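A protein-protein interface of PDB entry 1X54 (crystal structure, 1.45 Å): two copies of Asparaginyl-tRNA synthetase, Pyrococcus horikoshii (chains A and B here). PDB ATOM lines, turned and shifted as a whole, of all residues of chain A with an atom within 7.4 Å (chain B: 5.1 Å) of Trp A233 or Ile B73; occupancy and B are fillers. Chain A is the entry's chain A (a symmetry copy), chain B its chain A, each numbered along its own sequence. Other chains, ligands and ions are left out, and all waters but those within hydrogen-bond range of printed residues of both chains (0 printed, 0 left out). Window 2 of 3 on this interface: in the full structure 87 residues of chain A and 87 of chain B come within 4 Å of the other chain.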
ATOM      1  N   ILE A 197     -16.536  -7.996  17.494  1.00  0.00           N
ATOM      2  CA  ILE A 197     -15.990  -8.941  18.492  1.00  0.00           C
ATOM      3  C   ILE A 197     -15.408  -8.213  19.704  1.00  0.00           C
ATOM      4  O   ILE A 197     -15.306  -8.808  20.773  1.00  0.00           O
ATOM      5  CB  ILE A 197     -14.937  -9.904  17.917  1.00  0.00           C
ATOM      6  CG1 ILE A 197     -13.718  -9.111  17.451  1.00  0.00           C
ATOM      7  CG2 ILE A 197     -15.555 -10.796  16.864  1.00  0.00           C
ATOM      8  CD1 ILE A 197     -12.545  -9.962  16.976  1.00  0.00           C
ATOM      9  N   GLU A 201     -17.345 -10.478  21.585  1.00  0.00           N
ATOM     10  CA  GLU A 201     -16.405 -11.633  21.544  1.00  0.00           C
ATOM     11  C   GLU A 201     -16.676 -12.691  20.487  1.00  0.00           C
ATOM     12  O   GLU A 201     -15.782 -13.024  19.716  1.00  0.00           O
ATOM     13  CB  GLU A 201     -16.174 -12.286  22.910  1.00  0.00           C
ATOM     14  CG  GLU A 201     -15.388 -11.399  23.852  1.00  0.00           C
ATOM     15  CD  GLU A 201     -15.182 -12.098  25.169  1.00  0.00           C
ATOM     16  OE1 GLU A 201     -16.020 -11.890  26.067  1.00  0.00           O
ATOM     17  OE2 GLU A 201     -14.227 -12.919  25.280  1.00  0.00           O
ATOM     18  N   LYS A 202     -17.899 -13.222  20.459  1.00  0.00           N
ATOM     19  CA  LYS A 202     -18.283 -14.258  19.480  1.00  0.00           C
ATOM     20  C   LYS A 202     -19.545 -13.766  18.806  1.00  0.00           C
ATOM     21  O   LYS A 202     -20.573 -13.598  19.461  1.00  0.00           O
ATOM     22  CB  LYS A 202     -18.541 -15.595  20.177  1.00  0.00           C
ATOM     23  CG  LYS A 202     -17.266 -16.215  20.766  1.00  0.00           C
ATOM     24  CD  LYS A 202     -17.517 -17.359  21.730  1.00  0.00           C
ATOM     25  CE  LYS A 202     -18.280 -18.517  21.146  1.00  0.00           C
ATOM     26  NZ  LYS A 202     -18.342 -19.695  22.083  1.00  0.00           N
ATOM     27  N   ALA A 231     -14.681 -14.554  15.812  1.00  0.00           N
ATOM     28  CA  ALA A 231     -14.449 -14.772  17.255  1.00  0.00           C
ATOM     29  C   ALA A 231     -13.109 -14.242  17.710  1.00  0.00           C
ATOM     30  O   ALA A 231     -12.067 -14.600  17.155  1.00  0.00           O
ATOM     31  CB  ALA A 231     -14.522 -16.264  17.604  1.00  0.00           C
ATOM     32  N   ALA A 232     -13.144 -13.401  18.742  1.00  0.00           N
ATOM     33  CA  ALA A 232     -11.944 -13.057  19.493  1.00  0.00           C
ATOM     34  C   ALA A 232     -11.279 -14.328  20.042  1.00  0.00           C
ATOM     35  O   ALA A 232     -11.941 -15.331  20.365  1.00  0.00           O
ATOM     36  CB  ALA A 232     -12.303 -12.142  20.652  1.00  0.00           C
ATOM     37  N   TRP A 233      -9.951 -14.244  20.168  1.00  0.00           N
ATOM     38  CA  TRP A 233      -9.093 -15.232  20.850  1.00  0.00           C
ATOM     39  C   TRP A 233      -8.801 -16.474  20.038  1.00  0.00           C
ATOM     40  O   TRP A 233      -7.823 -17.170  20.314  1.00  0.00           O
ATOM     41  CB  TRP A 233      -9.604 -15.629  22.256  1.00  0.00           C
ATOM     42  CG  TRP A 233     -10.145 -14.495  23.049  1.00  0.00           C
ATOM     43  CD1 TRP A 233     -11.450 -14.311  23.417  1.00  0.00           C
ATOM     44  CD2 TRP A 233      -9.435 -13.337  23.500  1.00  0.00           C
ATOM     45  NE1 TRP A 233     -11.589 -13.125  24.087  1.00  0.00           N
ATOM     46  CE2 TRP A 233     -10.369 -12.500  24.154  1.00  0.00           C
ATOM     47  CE3 TRP A 233      -8.092 -12.919  23.427  1.00  0.00           C
ATOM     48  CZ2 TRP A 233     -10.008 -11.281  24.744  1.00  0.00           C
ATOM     49  CZ3 TRP A 233      -7.729 -11.702  24.025  1.00  0.00           C
ATOM     50  CH2 TRP A 233      -8.693 -10.899  24.673  1.00  0.00           C
ATOM     51  N   MET A 234      -9.621 -16.754  19.033  1.00  0.00           N
ATOM     52  CA  MET A 234      -9.490 -17.991  18.268  1.00  0.00           C
ATOM     53  C   MET A 234      -8.480 -17.860  17.157  1.00  0.00           C
ATOM     54  O   MET A 234      -8.478 -16.853  16.448  1.00  0.00           O
ATOM     55  CB  MET A 234     -10.846 -18.356  17.661  1.00  0.00           C
ATOM     56  CG  MET A 234     -11.845 -18.806  18.683  1.00  0.00           C
ATOM     57  SD  MET A 234     -13.170 -19.707  17.871  1.00  0.00           S
ATOM     58  CE  MET A 234     -14.338 -19.724  19.222  1.00  0.00           C
ATOM     59  N   ASP A 235      -7.654 -18.899  16.999  1.00  0.00           N
ATOM     60  CA  ASP A 235      -6.756 -18.990  15.851  1.00  0.00           C
ATOM     61  C   ASP A 235      -7.369 -19.836  14.736  1.00  0.00           C
ATOM     62  O   ASP A 235      -8.520 -20.267  14.836  1.00  0.00           O
ATOM     63  CB  ASP A 235      -5.364 -19.482  16.268  1.00  0.00           C
ATOM     64  CG  ASP A 235      -5.350 -20.914  16.763  1.00  0.00           C
ATOM     65  OD1 ASP A 235      -6.313 -21.684  16.529  1.00  0.00           O
ATOM     66  OD2 ASP A 235      -4.359 -21.350  17.415  1.00  0.00           O
ATOM     67  N   LEU A 236      -6.609 -20.063  13.675  1.00  0.00           N
ATOM     68  CA  LEU A 236      -7.151 -20.790  12.519  1.00  0.00           C
ATOM     69  C   LEU A 236      -7.648 -22.172  12.945  1.00  0.00           C
ATOM     70  O   LEU A 236      -8.713 -22.630  12.506  1.00  0.00           O
ATOM     71  CB  LEU A 236      -6.092 -20.929  11.420  1.00  0.00           C
ATOM     72  CG  LEU A 236      -6.523 -21.830  10.247  1.00  0.00           C
ATOM     73  CD1 LEU A 236      -7.664 -21.182   9.502  1.00  0.00           C
ATOM     74  CD2 LEU A 236      -5.337 -22.056   9.324  1.00  0.00           C
ATOM     75  N   ASP A 238      -8.654 -23.264  15.841  1.00  0.00           N
ATOM     76  CA  ASP A 238      -9.870 -23.129  16.629  1.00  0.00           C
ATOM     77  C   ASP A 238     -11.093 -22.905  15.742  1.00  0.00           C
ATOM     78  O   ASP A 238     -12.151 -23.541  15.942  1.00  0.00           O
ATOM     79  CB  ASP A 238      -9.741 -21.922  17.540  1.00  0.00           C
ATOM     80  CG  ASP A 238      -8.671 -22.084  18.573  1.00  0.00           C
ATOM     81  OD1 ASP A 238      -8.130 -21.034  18.992  1.00  0.00           O
ATOM     82  OD2 ASP A 238      -8.345 -23.204  19.035  1.00  0.00           O
ATOM     83  N   GLN A 363      -7.586 -17.026   9.871  1.00  0.00           N
ATOM     84  CA  GLN A 363      -7.166 -16.180  10.981  1.00  0.00           C
ATOM     85  C   GLN A 363      -6.837 -14.801  10.391  1.00  0.00           C
ATOM     86  O   GLN A 363      -6.339 -14.696   9.257  1.00  0.00           O
ATOM     87  CB  GLN A 363      -5.967 -16.771  11.714  1.00  0.00           C
ATOM     88  CG  GLN A 363      -5.609 -15.980  12.951  1.00  0.00           C
ATOM     89  CD  GLN A 363      -4.669 -16.696  13.873  1.00  0.00           C
ATOM     90  OE1 GLN A 363      -4.346 -17.887  13.678  1.00  0.00           O
ATOM     91  NE2 GLN A 363      -4.231 -15.984  14.900  1.00  0.00           N
ATOM     92  N   GLY A 395      -6.463  -2.115  21.158  1.00  0.00           N
ATOM     93  CA  GLY A 395      -6.637  -3.329  21.933  1.00  0.00           C
ATOM     94  C   GLY A 395      -6.779  -4.537  21.031  1.00  0.00           C
ATOM     95  O   GLY A 395      -7.671  -5.388  21.226  1.00  0.00           O
ATOM     96  N   SER A 396      -5.921  -4.592  20.012  1.00  0.00           N
ATOM     97  CA  SER A 396      -5.886  -5.730  19.101  1.00  0.00           C
ATOM     98  C   SER A 396      -5.850  -7.065  19.842  1.00  0.00           C
ATOM     99  O   SER A 396      -5.185  -7.205  20.887  1.00  0.00           O
ATOM    100  CB  SER A 396      -4.660  -5.625  18.192  1.00  0.00           C
ATOM    101  OG  SER A 396      -4.794  -6.542  17.126  1.00  0.00           O
ATOM    102  N   VAL A 397      -6.565  -8.052  19.306  1.00  0.00           N
ATOM    103  CA  VAL A 397      -6.480  -9.411  19.845  1.00  0.00           C
ATOM    104  C   VAL A 397      -6.419 -10.371  18.656  1.00  0.00           C
ATOM    105  O   VAL A 397      -6.898 -10.026  17.572  1.00  0.00           O
ATOM    106  CB  VAL A 397      -7.707  -9.795  20.748  1.00  0.00           C
ATOM    107  CG1 VAL A 397      -7.806  -8.854  21.966  1.00  0.00           C
ATOM    108  CG2 VAL A 397      -9.012  -9.798  19.944  1.00  0.00           C
ATOM    109  N   PRO A 398      -5.850 -11.568  18.844  1.00  0.00           N
ATOM    110  CA  PRO A 398      -5.907 -12.564  17.778  1.00  0.00           C
ATOM    111  C   PRO A 398      -7.370 -12.907  17.549  1.00  0.00           C
ATOM    112  O   PRO A 398      -8.148 -12.956  18.506  1.00  0.00           O
ATOM    113  CB  PRO A 398      -5.171 -13.776  18.348  1.00  0.00           C
ATOM    114  CG  PRO A 398      -4.571 -13.352  19.647  1.00  0.00           C
ATOM    115  CD  PRO A 398      -5.177 -12.059  20.064  1.00  0.00           C
ATOM    116  N   HIS A 399      -7.750 -13.143  16.298  1.00  0.00           N
ATOM    117  CA  HIS A 399      -9.129 -13.522  16.001  1.00  0.00           C
ATOM    118  C   HIS A 399      -9.210 -14.157  14.634  1.00  0.00           C
ATOM    119  O   HIS A 399      -8.322 -13.968  13.803  1.00  0.00           O
ATOM    120  CB  HIS A 399     -10.078 -12.314  16.127  1.00  0.00           C
ATOM    121  CG  HIS A 399      -9.779 -11.164  15.210  1.00  0.00           C
ATOM    122  ND1 HIS A 399      -8.812 -10.207  15.471  1.00  0.00           N
ATOM    123  CD2 HIS A 399     -10.390 -10.773  14.067  1.00  0.00           C
ATOM    124  CE1 HIS A 399      -8.831  -9.291  14.512  1.00  0.00           C
ATOM    125  NE2 HIS A 399      -9.773  -9.619  13.639  1.00  0.00           N
ATOM    126  N   SER A 400     -10.299 -14.890  14.414  1.00  0.00           N
ATOM    127  CA  SER A 400     -10.498 -15.666  13.196  1.00  0.00           C
ATOM    128  C   SER A 400     -11.992 -15.706  12.905  1.00  0.00           C
ATOM    129  O   SER A 400     -12.824 -15.458  13.777  1.00  0.00           O
ATOM    130  CB  SER A 400     -10.018 -17.104  13.397  1.00  0.00           C
ATOM    131  OG  SER A 400      -8.650 -17.125  13.738  1.00  0.00           O
ATOM    132  N   MET B   1      -7.131 -23.533  21.480  1.00  0.00           N
ATOM    133  CA  MET B   1      -7.243 -22.289  22.285  1.00  0.00           C
ATOM    134  C   MET B   1      -7.112 -22.605  23.760  1.00  0.00           C
ATOM    135  O   MET B   1      -7.768 -23.522  24.261  1.00  0.00           O
ATOM    136  CB  MET B   1      -8.597 -21.632  22.034  1.00  0.00           C
ATOM    137  CG  MET B   1      -8.882 -20.378  22.851  1.00  0.00           C
ATOM    138  SD  MET B   1     -10.367 -19.562  22.232  1.00  0.00           S
ATOM    139  CE  MET B   1     -11.414 -20.990  21.883  1.00  0.00           C
ATOM    140  N   LYS B   4     -10.639 -19.564  28.359  1.00  0.00           N
ATOM    141  CA  LYS B   4     -10.804 -18.419  29.254  1.00  0.00           C
ATOM    142  C   LYS B   4     -12.007 -18.608  30.168  1.00  0.00           C
ATOM    143  O   LYS B   4     -12.921 -19.402  29.893  1.00  0.00           O
ATOM    144  CB  LYS B   4     -10.929 -17.105  28.457  1.00  0.00           C
ATOM    145  CG  LYS B   4     -12.200 -16.999  27.564  1.00  0.00           C
ATOM    146  CD  LYS B   4     -12.496 -15.565  27.123  1.00  0.00           C
ATOM    147  CE  LYS B   4     -13.189 -14.815  28.247  1.00  0.00           C
ATOM    148  NZ  LYS B   4     -13.391 -13.384  27.920  1.00  0.00           N
ATOM    149  N   ARG B  20      -8.311 -17.756  34.118  1.00  0.00           N
ATOM    150  CA  ARG B  20      -7.633 -17.021  33.075  1.00  0.00           C
ATOM    151  C   ARG B  20      -8.654 -16.089  32.454  1.00  0.00           C
ATOM    152  O   ARG B  20      -9.573 -16.540  31.778  1.00  0.00           O
ATOM    153  CB  ARG B  20      -7.083 -17.999  32.039  1.00  0.00           C
ATOM    154  CG  ARG B  20      -6.329 -17.379  30.928  1.00  0.00           C
ATOM    155  CD  ARG B  20      -5.753 -18.439  29.985  1.00  0.00           C
ATOM    156  NE  ARG B  20      -5.173 -17.840  28.789  1.00  0.00           N
ATOM    157  CZ  ARG B  20      -5.874 -17.444  27.736  1.00  0.00           C
ATOM    158  NH1 ARG B  20      -7.198 -17.591  27.716  1.00  0.00           N
ATOM    159  NH2 ARG B  20      -5.250 -16.897  26.693  1.00  0.00           N
ATOM    160  N   LEU B  21      -8.508 -14.793  32.702  1.00  0.00           N
ATOM    161  CA  LEU B  21      -9.358 -13.790  32.052  1.00  0.00           C
ATOM    162  C   LEU B  21      -8.747 -13.334  30.748  1.00  0.00           C
ATOM    163  O   LEU B  21      -7.530 -13.310  30.611  1.00  0.00           O
ATOM    164  CB  LEU B  21      -9.507 -12.564  32.955  1.00  0.00           C
ATOM    165  CG  LEU B  21      -9.920 -12.818  34.402  1.00  0.00           C
ATOM    166  CD1 LEU B  21      -9.981 -11.475  35.100  1.00  0.00           C
ATOM    167  CD2 LEU B  21     -11.262 -13.531  34.470  1.00  0.00           C
ATOM    168  N   ALA B  22      -9.599 -12.917  29.811  1.00  0.00           N
ATOM    169  CA  ALA B  22      -9.124 -12.368  28.551  1.00  0.00           C
ATOM    170  C   ALA B  22     -10.082 -11.252  28.172  1.00  0.00           C
ATOM    171  O   ALA B  22     -11.288 -11.479  28.044  1.00  0.00           O
ATOM    172  CB  ALA B  22      -9.088 -13.431  27.480  1.00  0.00           C
ATOM    173  N   GLY B  23      -9.576 -10.033  28.080  1.00  0.00           N
ATOM    174  CA  GLY B  23     -10.455  -8.922  27.756  1.00  0.00           C
ATOM    175  C   GLY B  23      -9.700  -7.631  27.659  1.00  0.00           C
ATOM    176  O   GLY B  23      -8.548  -7.611  27.252  1.00  0.00           O
ATOM    177  N   TRP B  24     -10.374  -6.552  28.035  1.00  0.00           N
ATOM    178  CA  TRP B  24      -9.871  -5.197  27.800  1.00  0.00           C
ATOM    179  C   TRP B  24      -9.965  -4.368  29.064  1.00  0.00           C
ATOM    180  O   TRP B  24     -10.933  -4.457  29.810  1.00  0.00           O
ATOM    181  CB  TRP B  24     -10.679  -4.514  26.678  1.00  0.00           C
ATOM    182  CG  TRP B  24     -10.528  -5.213  25.345  1.00  0.00           C
ATOM    183  CD1 TRP B  24      -9.629  -4.914  24.368  1.00  0.00           C
ATOM    184  CD2 TRP B  24     -11.289  -6.334  24.853  1.00  0.00           C
ATOM    185  NE1 TRP B  24      -9.764  -5.778  23.306  1.00  0.00           N
ATOM    186  CE2 TRP B  24     -10.774  -6.665  23.576  1.00  0.00           C
ATOM    187  CE3 TRP B  24     -12.346  -7.091  25.363  1.00  0.00           C
ATOM    188  CZ2 TRP B  24     -11.286  -7.717  22.807  1.00  0.00           C
ATOM    189  CZ3 TRP B  24     -12.852  -8.169  24.599  1.00  0.00           C
ATOM    190  CH2 TRP B  24     -12.325  -8.459  23.337  1.00  0.00           C
ATOM    191  N   SER B  71      -5.641  -4.456  25.593  1.00  0.00           N
ATOM    192  CA  SER B  71      -6.015  -5.873  25.562  1.00  0.00           C
ATOM    193  C   SER B  71      -5.049  -6.683  26.403  1.00  0.00           C
ATOM    194  O   SER B  71      -3.823  -6.532  26.283  1.00  0.00           O
ATOM    195  CB  SER B  71      -6.094  -6.380  24.116  1.00  0.00           C
ATOM    196  OG  SER B  71      -4.913  -6.072  23.404  1.00  0.00           O
ATOM    197  N   VAL B  72      -5.605  -7.536  27.260  1.00  0.00           N
ATOM    198  CA  VAL B  72      -4.832  -8.278  28.258  1.00  0.00           C
ATOM    199  C   VAL B  72      -5.324  -9.700  28.477  1.00  0.00           C
ATOM    200  O   VAL B  72      -6.511  -9.989  28.295  1.00  0.00           O
ATOM    201  CB  VAL B  72      -4.832  -7.548  29.632  1.00  0.00           C
ATOM    202  CG1 VAL B  72      -4.113  -6.215  29.540  1.00  0.00           C
ATOM    203  CG2 VAL B  72      -6.243  -7.346  30.137  1.00  0.00           C
ATOM    204  N   ILE B  73      -4.394 -10.581  28.852  1.00  0.00           N
ATOM    205  CA  ILE B  73      -4.715 -11.873  29.449  1.00  0.00           C
ATOM    206  C   ILE B  73      -4.235 -11.822  30.877  1.00  0.00           C
ATOM    207  O   ILE B  73      -3.092 -11.407  31.131  1.00  0.00           O
ATOM    208  CB  ILE B  73      -3.959 -13.019  28.755  1.00  0.00           C
ATOM    209  CG1 ILE B  73      -4.184 -13.015  27.253  1.00  0.00           C
ATOM    210  CG2 ILE B  73      -4.303 -14.357  29.395  1.00  0.00           C
ATOM    211  CD1 ILE B  73      -5.595 -13.001  26.851  1.00  0.00           C
ATOM    212  N   VAL B  74      -5.090 -12.241  31.799  1.00  0.00           N
ATOM    213  CA  VAL B  74      -4.774 -12.189  33.218  1.00  0.00           C
ATOM    214  C   VAL B  74      -4.987 -13.573  33.818  1.00  0.00           C
ATOM    215  O   VAL B  74      -6.073 -14.127  33.701  1.00  0.00           O
ATOM    216  CB  VAL B  74      -5.701 -11.166  33.912  1.00  0.00           C
ATOM    217  CG1 VAL B  74      -5.483 -11.150  35.429  1.00  0.00           C
ATOM    218  CG2 VAL B  74      -5.517  -9.762  33.282  1.00  0.00           C
ATOM    219  N   GLU B  75      -3.961 -14.145  34.445  1.00  0.00           N
ATOM    220  CA  GLU B  75      -4.150 -15.381  35.191  1.00  0.00           C
ATOM    221  C   GLU B  75      -3.998 -15.062  36.666  1.00  0.00           C
ATOM    222  O   GLU B  75      -3.088 -14.317  37.055  1.00  0.00           O
ATOM    223  CB  GLU B  75      -3.139 -16.436  34.754  1.00  0.00           C
ATOM    224  CG  GLU B  75      -3.416 -16.977  33.356  1.00  0.00           C
ATOM    225  CD  GLU B  75      -2.428 -18.043  32.918  1.00  0.00           C
ATOM    226  OE1 GLU B  75      -2.555 -18.532  31.760  1.00  0.00           O
ATOM    227  OE2 GLU B  75      -1.528 -18.397  33.724  1.00  0.00           O
ATOM    228  N   LYS B  94      -0.138 -13.650  36.809  1.00  0.00           N
ATOM    229  CA  LYS B  94       0.485 -13.405  35.512  1.00  0.00           C
ATOM    230  C   LYS B  94      -0.351 -12.396  34.728  1.00  0.00           C
ATOM    231  O   LYS B  94      -1.564 -12.531  34.650  1.00  0.00           O
ATOM    232  CB  LYS B  94       0.589 -14.714  34.721  1.00  0.00           C
ATOM    233  CG  LYS B  94       1.418 -14.650  33.460  1.00  0.00           C
ATOM    234  CD  LYS B  94       0.587 -14.401  32.190  1.00  0.00           C
ATOM    235  CE  LYS B  94       1.229 -15.038  30.939  1.00  0.00           C
ATOM    236  NZ  LYS B  94       2.716 -14.841  30.846  1.00  0.00           N
ATOM    237  N   LEU B  95       0.309 -11.401  34.152  1.00  0.00           N
ATOM    238  CA  LEU B  95      -0.344 -10.438  33.271  1.00  0.00           C
ATOM    239  C   LEU B  95       0.382 -10.431  31.937  1.00  0.00           C
ATOM    240  O   LEU B  95       1.583 -10.157  31.897  1.00  0.00           O
ATOM    241  CB  LEU B  95      -0.321  -9.044  33.913  1.00  0.00           C
ATOM    242  CG  LEU B  95      -0.725  -7.813  33.084  1.00  0.00           C
ATOM    243  CD1 LEU B  95      -2.220  -7.814  32.677  1.00  0.00           C
ATOM    244  CD2 LEU B  95      -0.390  -6.542  33.864  1.00  0.00           C
ATOM    245  N   GLU B  96      -0.332 -10.761  30.861  1.00  0.00           N
ATOM    246  CA  GLU B  96       0.178 -10.650  29.504  1.00  0.00           C
ATOM    247  C   GLU B  96      -0.513  -9.470  28.860  1.00  0.00           C
ATOM    248  O   GLU B  96      -1.747  -9.455  28.693  1.00  0.00           O
ATOM    249  CB  GLU B  96      -0.100 -11.925  28.678  1.00  0.00           C
ATOM    250  CG  GLU B  96       0.449 -11.876  27.257  1.00  0.00           C
ATOM    251  CD  GLU B  96      -0.051 -13.004  26.368  1.00  0.00           C
ATOM    252  OE1 GLU B  96      -0.040 -12.820  25.120  1.00  0.00           O
ATOM    253  OE2 GLU B  96      -0.446 -14.079  26.893  1.00  0.00           O
ATOM    254  N   ILE B  98      -1.357  -7.729  25.672  1.00  0.00           N
ATOM    255  CA  ILE B  98      -1.393  -7.976  24.237  1.00  0.00           C
ATOM    256  C   ILE B  98      -1.120  -6.675  23.501  1.00  0.00           C
ATOM    257  O   ILE B  98      -0.169  -6.584  22.708  1.00  0.00           O
ATOM    258  CB  ILE B  98      -2.723  -8.605  23.796  1.00  0.00           C
ATOM    259  CG1 ILE B  98      -2.923  -9.928  24.532  1.00  0.00           C
ATOM    260  CG2 ILE B  98      -2.716  -8.817  22.272  1.00  0.00           C
ATOM    261  CD1 ILE B  98      -4.305 -10.533  24.324  1.00  0.00           C
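OD2 of Asp A238 sits at hydrogen-bond distance from N of Met B1 (2.7 Å).
The side-chain carboxylate of Glu A201 lies within salt-bridge range of the side-chain amino group of Lys B4.
NE1 of Trp B24 is in hydrogen-bond range of O of Gly A395.
The side-chain hydroxyl of Ser B71 sits at hydrogen-bond distance from the backbone carbonyl oxygen of Ser A396 (2.8 Å).
The side-chain amino group of Lys B4 is in hydrogen-bond range of the backbone carbonyl oxygen of Ala B22 (2.8 Å).
The backbone carbonyl oxygen (O) of Ile B73 sits at hydrogen-bond distance from the backbone NH (N) of Glu B96 (2.8 Å).
NE1 of Trp A233 lies within hydrogen-bond range of OE2 of Glu A201 (2.9 Å).
O of Pro A398 is in hydrogen-bond range of N of Trp A233.
The backbone carbonyl oxygen (O) of Met A234 lies within hydrogen-bond range of the side-chain hydroxyl (OG) of Ser A400, at 2.7 Å.
The side-chain carboxylate (OD1) of Asp A235 lies within hydrogen-bond range of the backbone NH (N) of Asp A238 (2.9 Å).
Trp B24 touches Ile A197 (CH2 to O, 3.9 Å).
Trp A233 touches Met B1 (O to SD, 3.98 Å).
Lys B4 touches Trp A233 (CD to NE1, 3.999 Å).
Trp A233 touches Ala B22.
Gly B23 touches Trp A233.
Ile B73 touches Trp A233 (CD1 to CZ3, 3.8 Å).
CZ3 of Trp A233 touches CD1 of Ile B98 (3.6 Å).
Met A234 touches Met B1 (CG to CE, 3.9 Å).
Gly A395 touches Ser B71 (C to OG, 3.4 Å).
Val A397 touches Trp B24.
Printed residues of chain B within 4 Å of Trp A233: Met B1 (3.98 Å), Lys B4 (3.999 Å), Ala B22 (3.4 Å), Gly B23 (3.6 Å), Trp B24 (3.9 Å), Ile B73 (3.8 Å) and Ile B98 (3.6 Å).
Of the printed residues of chain B, Gly A395 touches Trp B24 and Ser B71.
Of the printed residues of chain A, Ala B22 touches Trp A233 (3.4 Å).
Printed residues of chain A within 4 Å of Ser B71: Gly A395 (3.4 Å), Ser A396 (2.8 Å) and Val A397 (3.7 Å).
Of chain A, only Trp A233 (3.8 Å) comes within 4 Å of Ile B73.
Printed residues of chain B that touch a printed residue of chain A: Met B1, Lys B4, Ala B22, Gly B23, Trp B24, Ser B71, Ile B73 and Ile B98.
Hydrophobic or aromatic side chains of chain B within 4 Å of the printed part of chain A: Met B1, Ala B22, Trp B24, Ile B73 and Ile B98.
Printed residues of chain A that touch a printed residue of chain B: Ile A197, Glu A201, Trp A233, Met A234, Asp A238, Gly A395, Ser A396 and Val A397.
Hydrophobic or aromatic side chains of chain A that line the printed part of chain B: Trp A233, Met A234 and Val A397.
Among the printed residues, 17 pairs touch across the chains.
Among the printed residues, Asp or Glu carboxylates within 4 Å of a Lys or Arg side-chain nitrogen of the other chain: Glu A201 with Lys B4 (2.8 Å).
No position is printed for both chains.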
